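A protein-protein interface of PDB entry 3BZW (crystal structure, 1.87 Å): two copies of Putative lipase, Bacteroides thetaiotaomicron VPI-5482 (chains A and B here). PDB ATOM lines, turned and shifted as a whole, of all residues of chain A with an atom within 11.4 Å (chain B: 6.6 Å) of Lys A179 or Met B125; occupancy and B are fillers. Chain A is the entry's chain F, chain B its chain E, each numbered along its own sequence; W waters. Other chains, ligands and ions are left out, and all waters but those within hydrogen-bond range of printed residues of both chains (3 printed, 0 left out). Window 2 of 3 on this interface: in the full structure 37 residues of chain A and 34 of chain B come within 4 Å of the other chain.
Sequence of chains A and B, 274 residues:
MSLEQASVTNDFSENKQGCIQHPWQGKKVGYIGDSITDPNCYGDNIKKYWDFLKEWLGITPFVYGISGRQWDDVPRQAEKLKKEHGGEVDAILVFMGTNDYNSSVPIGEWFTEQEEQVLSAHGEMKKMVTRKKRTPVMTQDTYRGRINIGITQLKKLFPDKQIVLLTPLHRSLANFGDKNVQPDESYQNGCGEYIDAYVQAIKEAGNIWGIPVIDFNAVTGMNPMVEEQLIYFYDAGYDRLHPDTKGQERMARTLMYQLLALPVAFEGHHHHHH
The backbone carbonyl oxygen of Ala B121 is in hydrogen-bond range of the backbone NH of Val A181 (2.9 Å).
A ring nitrogen (NE2) of His B122 sits at hydrogen-bond distance from the side-chain amide oxygen (OD1) of Asn A102, 2.8 Å away.
The backbone carbonyl oxygen of Lys A179 is in hydrogen-bond range of the backbone NH of Gly B123.
The side-chain amino group (NZ) of Lys B126 lies within salt-bridge range of the side-chain carboxylate (OD1) of Asp A178.
The backbone carbonyl oxygen (O) of Lys A179 sits close to the backbone carbonyl oxygen (O) of Ala B121 (3.4 Å).
A ring nitrogen (ND1) of His B122 sits close to the side-chain hydroxyl of Ser B120 (3.4 Å).
The backbone NH (N) of Ser B120 is in hydrogen-bond range of the backbone carbonyl oxygen (O) of Lys B127 (3.1 Å).
The side-chain amide oxygen of Gln A182 sits close to the side-chain amide oxygen of Asn A102 (3.4 Å).
OD1 of Asn A180 is in hydrogen-bond range of NE2 of Gln A182 (3.0 Å).
O of Asp A178 touches CB of Ala B121, 3.6 Å away.
Glu B124 touches Asp A178.
O of Asp A178 touches C of Met B125, at 3.5 Å.
Lys A179 touches His B122 (O to N, 3.6 Å).
Lys A179 touches Glu B124.
Lys A179 touches Met B125 (CG to N, 3.9 Å).
Asn A180 touches Ala B121.
O of Val A181 touches CA of Ser B120, at 3.6 Å.
O of Val A181 touches CE1 of His B122 (3.6 Å).
CG2 of Val A181 touches CE of Lys B126, 3.96 Å away.
Printed residues of chain B within 4 Å of Asn A102: His B122.
Of the printed residues of chain B, Asp A178 touches Ala B121, Glu B124, Met B125 and Lys B126.
Of the printed residues of chain B, Lys A179 touches Ala B121, His B122, Gly B123, Glu B124 and Met B125.
Printed residues of chain B within 4 Å of Asn A180: Ala B121 (3.4 Å).
Of the printed residues of chain B, Val A181 touches Ser B120, Ala B121, His B122 and Lys B126.
Of the printed residues of chain A, Ser B120 touches Val A181.
Ala B121 touches four residues of chain A.
Of chain A, only Lys A179 comes within 4 Å of Gly B123.
Printed residues of chain A within 4 Å of Met B125: Asp A178 and Lys A179.
Of chain A, only Asp A178 and Val A181 come within 4 Å of Lys B126.
The nearest residue of chain B that does not touch Lys A179 is Lys B126 (4.8 Å).
The nearest printed residue of chain B that does not touch Asn A180 is His B122 (5.1 Å).
Hydrophobic or aromatic side chains of chain A that line the printed part of chain B: Val A181.
Of the 8 printed residues of chain B, 7 touch a printed residue of chain A.
Hydrophobic or aromatic side chains of chain B that line the printed part of chain A: Ala B121, His B122 and Met B125.
Among the printed residues, 15 pairs touch across the chains.
Among the printed residues, Asp or Glu carboxylates within 4 Å of a Lys or Arg side-chain nitrogen of the other chain: Asp A178 with Lys B126 (2.5 Å).
No position is printed for both chains.
Of the 15 pairs that touch across the chains among the printed residues, none has its exchanged pair printed and touching as well.
Water W1 lies within hydrogen-bond range of the backbone carbonyl oxygen of Asn A102 (2.7 Å) and a ring nitrogen (NE2) of His B122 (3.4 Å).
Water W2 bridges the side-chain amide oxygen (OD1) of Asn A102 (2.8 Å) and a ring nitrogen (NE2) of His B122 (3.3 Å).
Water W3 lies within hydrogen-bond range of the side-chain amide oxygen of Asn A180, the backbone carbonyl oxygen of Ala B121 and the side-chain amide nitrogen of Asn A102.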
ATOM      1  N   ASN A 102       1.613  -2.091 -34.472  1.00  0.00           N
ATOM      2  CA  ASN A 102       2.004  -2.278 -33.083  1.00  0.00           C
ATOM      3  C   ASN A 102       0.934  -1.853 -32.085  1.00  0.00           C
ATOM      4  O   ASN A 102       0.817  -2.450 -31.018  1.00  0.00           O
ATOM      5  CB  ASN A 102       3.303  -1.528 -32.779  1.00  0.00           C
ATOM      6  CG  ASN A 102       3.807  -1.803 -31.372  1.00  0.00           C
ATOM      7  OD1 ASN A 102       3.988  -2.958 -30.986  1.00  0.00           O
ATOM      8  ND2 ASN A 102       4.031  -0.744 -30.599  1.00  0.00           N
ATOM      9  N   SER A 103       0.156  -0.833 -32.437  1.00  0.00           N
ATOM     10  CA  SER A 103      -0.893  -0.330 -31.554  1.00  0.00           C
ATOM     11  C   SER A 103      -2.222  -1.055 -31.723  1.00  0.00           C
ATOM     12  O   SER A 103      -3.244  -0.622 -31.197  1.00  0.00           O
ATOM     13  CB  SER A 103      -1.090   1.170 -31.780  1.00  0.00           C
ATOM     14  OG  SER A 103       0.113   1.861 -31.508  1.00  0.00           O
ATOM     15  N   ALA A 174      11.380  -5.629 -30.371  1.00  0.00           N
ATOM     16  CA  ALA A 174      11.813  -4.314 -29.911  1.00  0.00           C
ATOM     17  C   ALA A 174      11.363  -4.134 -28.464  1.00  0.00           C
ATOM     18  O   ALA A 174      10.167  -4.105 -28.180  1.00  0.00           O
ATOM     19  CB  ALA A 174      11.213  -3.221 -30.794  1.00  0.00           C
ATOM     20  N   ASN A 175      12.326  -4.009 -27.556  1.00  0.00           N
ATOM     21  CA  ASN A 175      12.023  -3.848 -26.140  1.00  0.00           C
ATOM     22  C   ASN A 175      12.621  -2.565 -25.570  1.00  0.00           C
ATOM     23  O   ASN A 175      13.840  -2.440 -25.456  1.00  0.00           O
ATOM     24  CB  ASN A 175      12.548  -5.053 -25.361  1.00  0.00           C
ATOM     25  CG  ASN A 175      12.031  -6.371 -25.910  1.00  0.00           C
ATOM     26  OD1 ASN A 175      10.839  -6.514 -26.193  1.00  0.00           O
ATOM     27  ND2 ASN A 175      12.922  -7.344 -26.055  1.00  0.00           N
ATOM     28  N   PHE A 176      11.756  -1.619 -25.212  1.00  0.00           N
ATOM     29  CA  PHE A 176      12.198  -0.343 -24.651  1.00  0.00           C
ATOM     30  C   PHE A 176      11.559  -0.102 -23.281  1.00  0.00           C
ATOM     31  O   PHE A 176      10.748   0.811 -23.118  1.00  0.00           O
ATOM     32  CB  PHE A 176      11.821   0.820 -25.579  1.00  0.00           C
ATOM     33  CG  PHE A 176      12.043   0.538 -27.041  1.00  0.00           C
ATOM     34  CD1 PHE A 176      11.013   0.032 -27.827  1.00  0.00           C
ATOM     35  CD2 PHE A 176      13.276   0.786 -27.633  1.00  0.00           C
ATOM     36  CE1 PHE A 176      11.207  -0.223 -29.187  1.00  0.00           C
ATOM     37  CE2 PHE A 176      13.483   0.534 -28.993  1.00  0.00           C
ATOM     38  CZ  PHE A 176      12.446   0.030 -29.768  1.00  0.00           C
ATOM     39  N   GLY A 177      11.918  -0.918 -22.299  1.00  0.00           N
ATOM     40  CA  GLY A 177      11.351  -0.747 -20.973  1.00  0.00           C
ATOM     41  C   GLY A 177      10.199  -1.694 -20.706  1.00  0.00           C
ATOM     42  O   GLY A 177       9.690  -2.335 -21.623  1.00  0.00           O
ATOM     43  N   ASP A 178       9.775  -1.771 -19.449  1.00  0.00           N
ATOM     44  CA  ASP A 178       8.691  -2.665 -19.054  1.00  0.00           C
ATOM     45  C   ASP A 178       7.303  -2.302 -19.573  1.00  0.00           C
ATOM     46  O   ASP A 178       6.371  -3.093 -19.444  1.00  0.00           O
ATOM     47  CB  ASP A 178       8.646  -2.785 -17.529  1.00  0.00           C
ATOM     48  CG  ASP A 178       9.894  -3.436 -16.961  1.00  0.00           C
ATOM     49  OD1 ASP A 178      10.759  -3.863 -17.754  1.00  0.00           O
ATOM     50  OD2 ASP A 178      10.006  -3.529 -15.721  1.00  0.00           O
ATOM     51  N   LYS A 179       7.157  -1.116 -20.156  1.00  0.00           N
ATOM     52  CA  LYS A 179       5.859  -0.705 -20.683  1.00  0.00           C
ATOM     53  C   LYS A 179       5.861  -0.602 -22.207  1.00  0.00           C
ATOM     54  O   LYS A 179       4.876  -0.172 -22.808  1.00  0.00           O
ATOM     55  CB  LYS A 179       5.434   0.636 -20.074  1.00  0.00           C
ATOM     56  CG  LYS A 179       5.034   0.559 -18.609  1.00  0.00           C
ATOM     57  CD  LYS A 179       4.594   1.925 -18.084  1.00  0.00           C
ATOM     58  CE  LYS A 179       4.036   1.827 -16.669  1.00  0.00           C
ATOM     59  NZ  LYS A 179       3.581   3.151 -16.151  1.00  0.00           N
ATOM     60  N   ASN A 180       6.966  -1.005 -22.826  1.00  0.00           N
ATOM     61  CA  ASN A 180       7.083  -0.953 -24.283  1.00  0.00           C
ATOM     62  C   ASN A 180       7.793  -2.211 -24.766  1.00  0.00           C
ATOM     63  O   ASN A 180       9.015  -2.226 -24.912  1.00  0.00           O
ATOM     64  CB  ASN A 180       7.886   0.278 -24.708  1.00  0.00           C
ATOM     65  CG  ASN A 180       7.756   0.582 -26.191  1.00  0.00           C
ATOM     66  OD1 ASN A 180       7.469  -0.302 -27.002  1.00  0.00           O
ATOM     67  ND2 ASN A 180       7.987   1.837 -26.555  1.00  0.00           N
ATOM     68  N   VAL A 181       7.020  -3.266 -24.998  1.00  0.00           N
ATOM     69  CA  VAL A 181       7.562  -4.538 -25.458  1.00  0.00           C
ATOM     70  C   VAL A 181       6.790  -4.952 -26.701  1.00  0.00           C
ATOM     71  O   VAL A 181       5.583  -5.196 -26.648  1.00  0.00           O
ATOM     72  CB  VAL A 181       7.425  -5.619 -24.367  1.00  0.00           C
ATOM     73  CG1 VAL A 181       8.000  -6.945 -24.854  1.00  0.00           C
ATOM     74  CG2 VAL A 181       8.148  -5.165 -23.114  1.00  0.00           C
ATOM     75  N   GLN A 182       7.499  -5.021 -27.820  1.00  0.00           N
ATOM     76  CA  GLN A 182       6.887  -5.363 -29.096  1.00  0.00           C
ATOM     77  C   GLN A 182       7.411  -6.680 -29.663  1.00  0.00           C
ATOM     78  O   GLN A 182       8.584  -6.785 -30.022  1.00  0.00           O
ATOM     79  CB  GLN A 182       7.157  -4.240 -30.098  1.00  0.00           C
ATOM     80  CG  GLN A 182       6.703  -2.860 -29.635  1.00  0.00           C
ATOM     81  CD  GLN A 182       7.163  -1.746 -30.573  1.00  0.00           C
ATOM     82  OE1 GLN A 182       7.129  -1.894 -31.791  1.00  0.00           O
ATOM     83  NE2 GLN A 182       7.584  -0.622 -30.001  1.00  0.00           N
ATOM     84  N   PRO A 183       6.547  -7.705 -29.738  1.00  0.00           N
ATOM     85  CA  PRO A 183       6.928  -9.019 -30.271  1.00  0.00           C
ATOM     86  C   PRO A 183       7.247  -8.907 -31.763  1.00  0.00           C
ATOM     87  O   PRO A 183       6.710  -8.029 -32.446  1.00  0.00           O
ATOM     88  CB  PRO A 183       5.684  -9.864 -30.016  1.00  0.00           C
ATOM     89  CG  PRO A 183       5.091  -9.233 -28.784  1.00  0.00           C
ATOM     90  CD  PRO A 183       5.218  -7.765 -29.104  1.00  0.00           C
ATOM     91  N   SER B 120       4.224  -8.898 -23.943  1.00  0.00           N
ATOM     92  CA  SER B 120       3.833  -7.718 -24.708  1.00  0.00           C
ATOM     93  C   SER B 120       3.520  -6.548 -23.779  1.00  0.00           C
ATOM     94  O   SER B 120       3.065  -6.747 -22.652  1.00  0.00           O
ATOM     95  CB  SER B 120       2.605  -8.042 -25.565  1.00  0.00           C
ATOM     96  OG  SER B 120       2.276  -6.962 -26.422  1.00  0.00           O
ATOM     97  N   ALA B 121       3.759  -5.328 -24.254  1.00  0.00           N
ATOM     98  CA  ALA B 121       3.495  -4.136 -23.452  1.00  0.00           C
ATOM     99  C   ALA B 121       3.314  -2.897 -24.319  1.00  0.00           C
ATOM    100  O   ALA B 121       4.170  -2.572 -25.138  1.00  0.00           O
ATOM    101  CB  ALA B 121       4.636  -3.912 -22.457  1.00  0.00           C
ATOM    102  N   HIS B 122       2.193  -2.206 -24.131  1.00  0.00           N
ATOM    103  CA  HIS B 122       1.897  -0.997 -24.892  1.00  0.00           C
ATOM    104  C   HIS B 122       1.294   0.082 -23.998  1.00  0.00           C
ATOM    105  O   HIS B 122       0.140   0.471 -24.170  1.00  0.00           O
ATOM    106  CB  HIS B 122       0.935  -1.325 -26.036  1.00  0.00           C
ATOM    107  CG  HIS B 122       1.493  -2.306 -27.017  1.00  0.00           C
ATOM    108  ND1 HIS B 122       1.724  -3.628 -26.698  1.00  0.00           N
ATOM    109  CD2 HIS B 122       1.914  -2.148 -28.293  1.00  0.00           C
ATOM    110  CE1 HIS B 122       2.265  -4.241 -27.736  1.00  0.00           C
ATOM    111  NE2 HIS B 122       2.392  -3.365 -28.717  1.00  0.00           N
ATOM    112  N   GLY B 123       2.083   0.558 -23.040  1.00  0.00           N
ATOM    113  CA  GLY B 123       1.600   1.589 -22.138  1.00  0.00           C
ATOM    114  C   GLY B 123       1.565   1.144 -20.689  1.00  0.00           C
ATOM    115  O   GLY B 123       1.806   1.946 -19.785  1.00  0.00           O
ATOM    116  N   GLU B 124       1.266  -0.132 -20.463  1.00  0.00           N
ATOM    117  CA  GLU B 124       1.204  -0.671 -19.107  1.00  0.00           C
ATOM    118  C   GLU B 124       2.291  -1.712 -18.868  1.00  0.00           C
ATOM    119  O   GLU B 124       3.005  -2.103 -19.792  1.00  0.00           O
ATOM    120  CB  GLU B 124      -0.168  -1.299 -18.850  1.00  0.00           C
ATOM    121  CG  GLU B 124      -1.328  -0.319 -18.915  1.00  0.00           C
ATOM    122  CD  GLU B 124      -2.666  -0.976 -18.623  1.00  0.00           C
ATOM    123  OE1 GLU B 124      -3.693  -0.263 -18.630  1.00  0.00           O
ATOM    124  OE2 GLU B 124      -2.692  -2.205 -18.388  1.00  0.00           O
ATOM    125  N   MET B 125       2.408  -2.159 -17.620  1.00  0.00           N
ATOM    126  CA  MET B 125       3.402  -3.157 -17.246  1.00  0.00           C
ATOM    127  C   MET B 125       3.314  -4.367 -18.171  1.00  0.00           C
ATOM    128  O   MET B 125       2.229  -4.897 -18.404  1.00  0.00           O
ATOM    129  CB  MET B 125       3.173  -3.609 -15.800  1.00  0.00           C
ATOM    130  CG  MET B 125       4.360  -3.392 -14.878  1.00  0.00           C
ATOM    131  SD  MET B 125       5.957  -4.264 -15.512  1.00  0.00           S
ATOM    132  CE  MET B 125       5.641  -6.039 -14.818  1.00  0.00           C
ATOM    133  N   LYS B 126       4.459  -4.801 -18.687  1.00  0.00           N
ATOM    134  CA  LYS B 126       4.513  -5.947 -19.583  1.00  0.00           C
ATOM    135  C   LYS B 126       3.829  -7.158 -18.952  1.00  0.00           C
ATOM    136  O   LYS B 126       3.955  -7.398 -17.750  1.00  0.00           O
ATOM    137  CB  LYS B 126       5.967  -6.302 -19.907  1.00  0.00           C
ATOM    138  CG  LYS B 126       6.765  -6.792 -18.700  1.00  0.00           C
ATOM    139  CD  LYS B 126       8.004  -7.570 -19.121  1.00  0.00           C
ATOM    140  CE  LYS B 126       9.131  -6.668 -19.584  1.00  0.00           C
ATOM    141  NZ  LYS B 126       9.863  -6.082 -18.426  1.00  0.00           N
ATOM    142  N   LYS B 127       3.101  -7.913 -19.766  1.00  0.00           N
ATOM    143  CA  LYS B 127       2.410  -9.104 -19.288  1.00  0.00           C
ATOM    144  C   LYS B 127       2.430 -10.192 -20.350  1.00  0.00           C
ATOM    145  O   LYS B 127       2.649  -9.919 -21.531  1.00  0.00           O
ATOM    146  CB  LYS B 127       0.959  -8.776 -18.924  1.00  0.00           C
ATOM    147  CG  LYS B 127       0.817  -7.793 -17.773  1.00  0.00           C
ATOM    148  CD  LYS B 127      -0.642  -7.558 -17.419  1.00  0.00           C
ATOM    149  CE  LYS B 127      -0.775  -6.619 -16.226  1.00  0.00           C
ATOM    150  NZ  LYS B 127      -2.196  -6.455 -15.798  1.00  0.00           N
HETATM  151  O   HOH W   1      -1.026  -3.179 -29.135  1.00  0.00           O
HETATM  152  O   HOH W   2       2.948  -5.509 -31.099  1.00  0.00           O
HETATM  153  O   HOH W   3       4.862  -1.115 -27.471  1.00  0.00           O
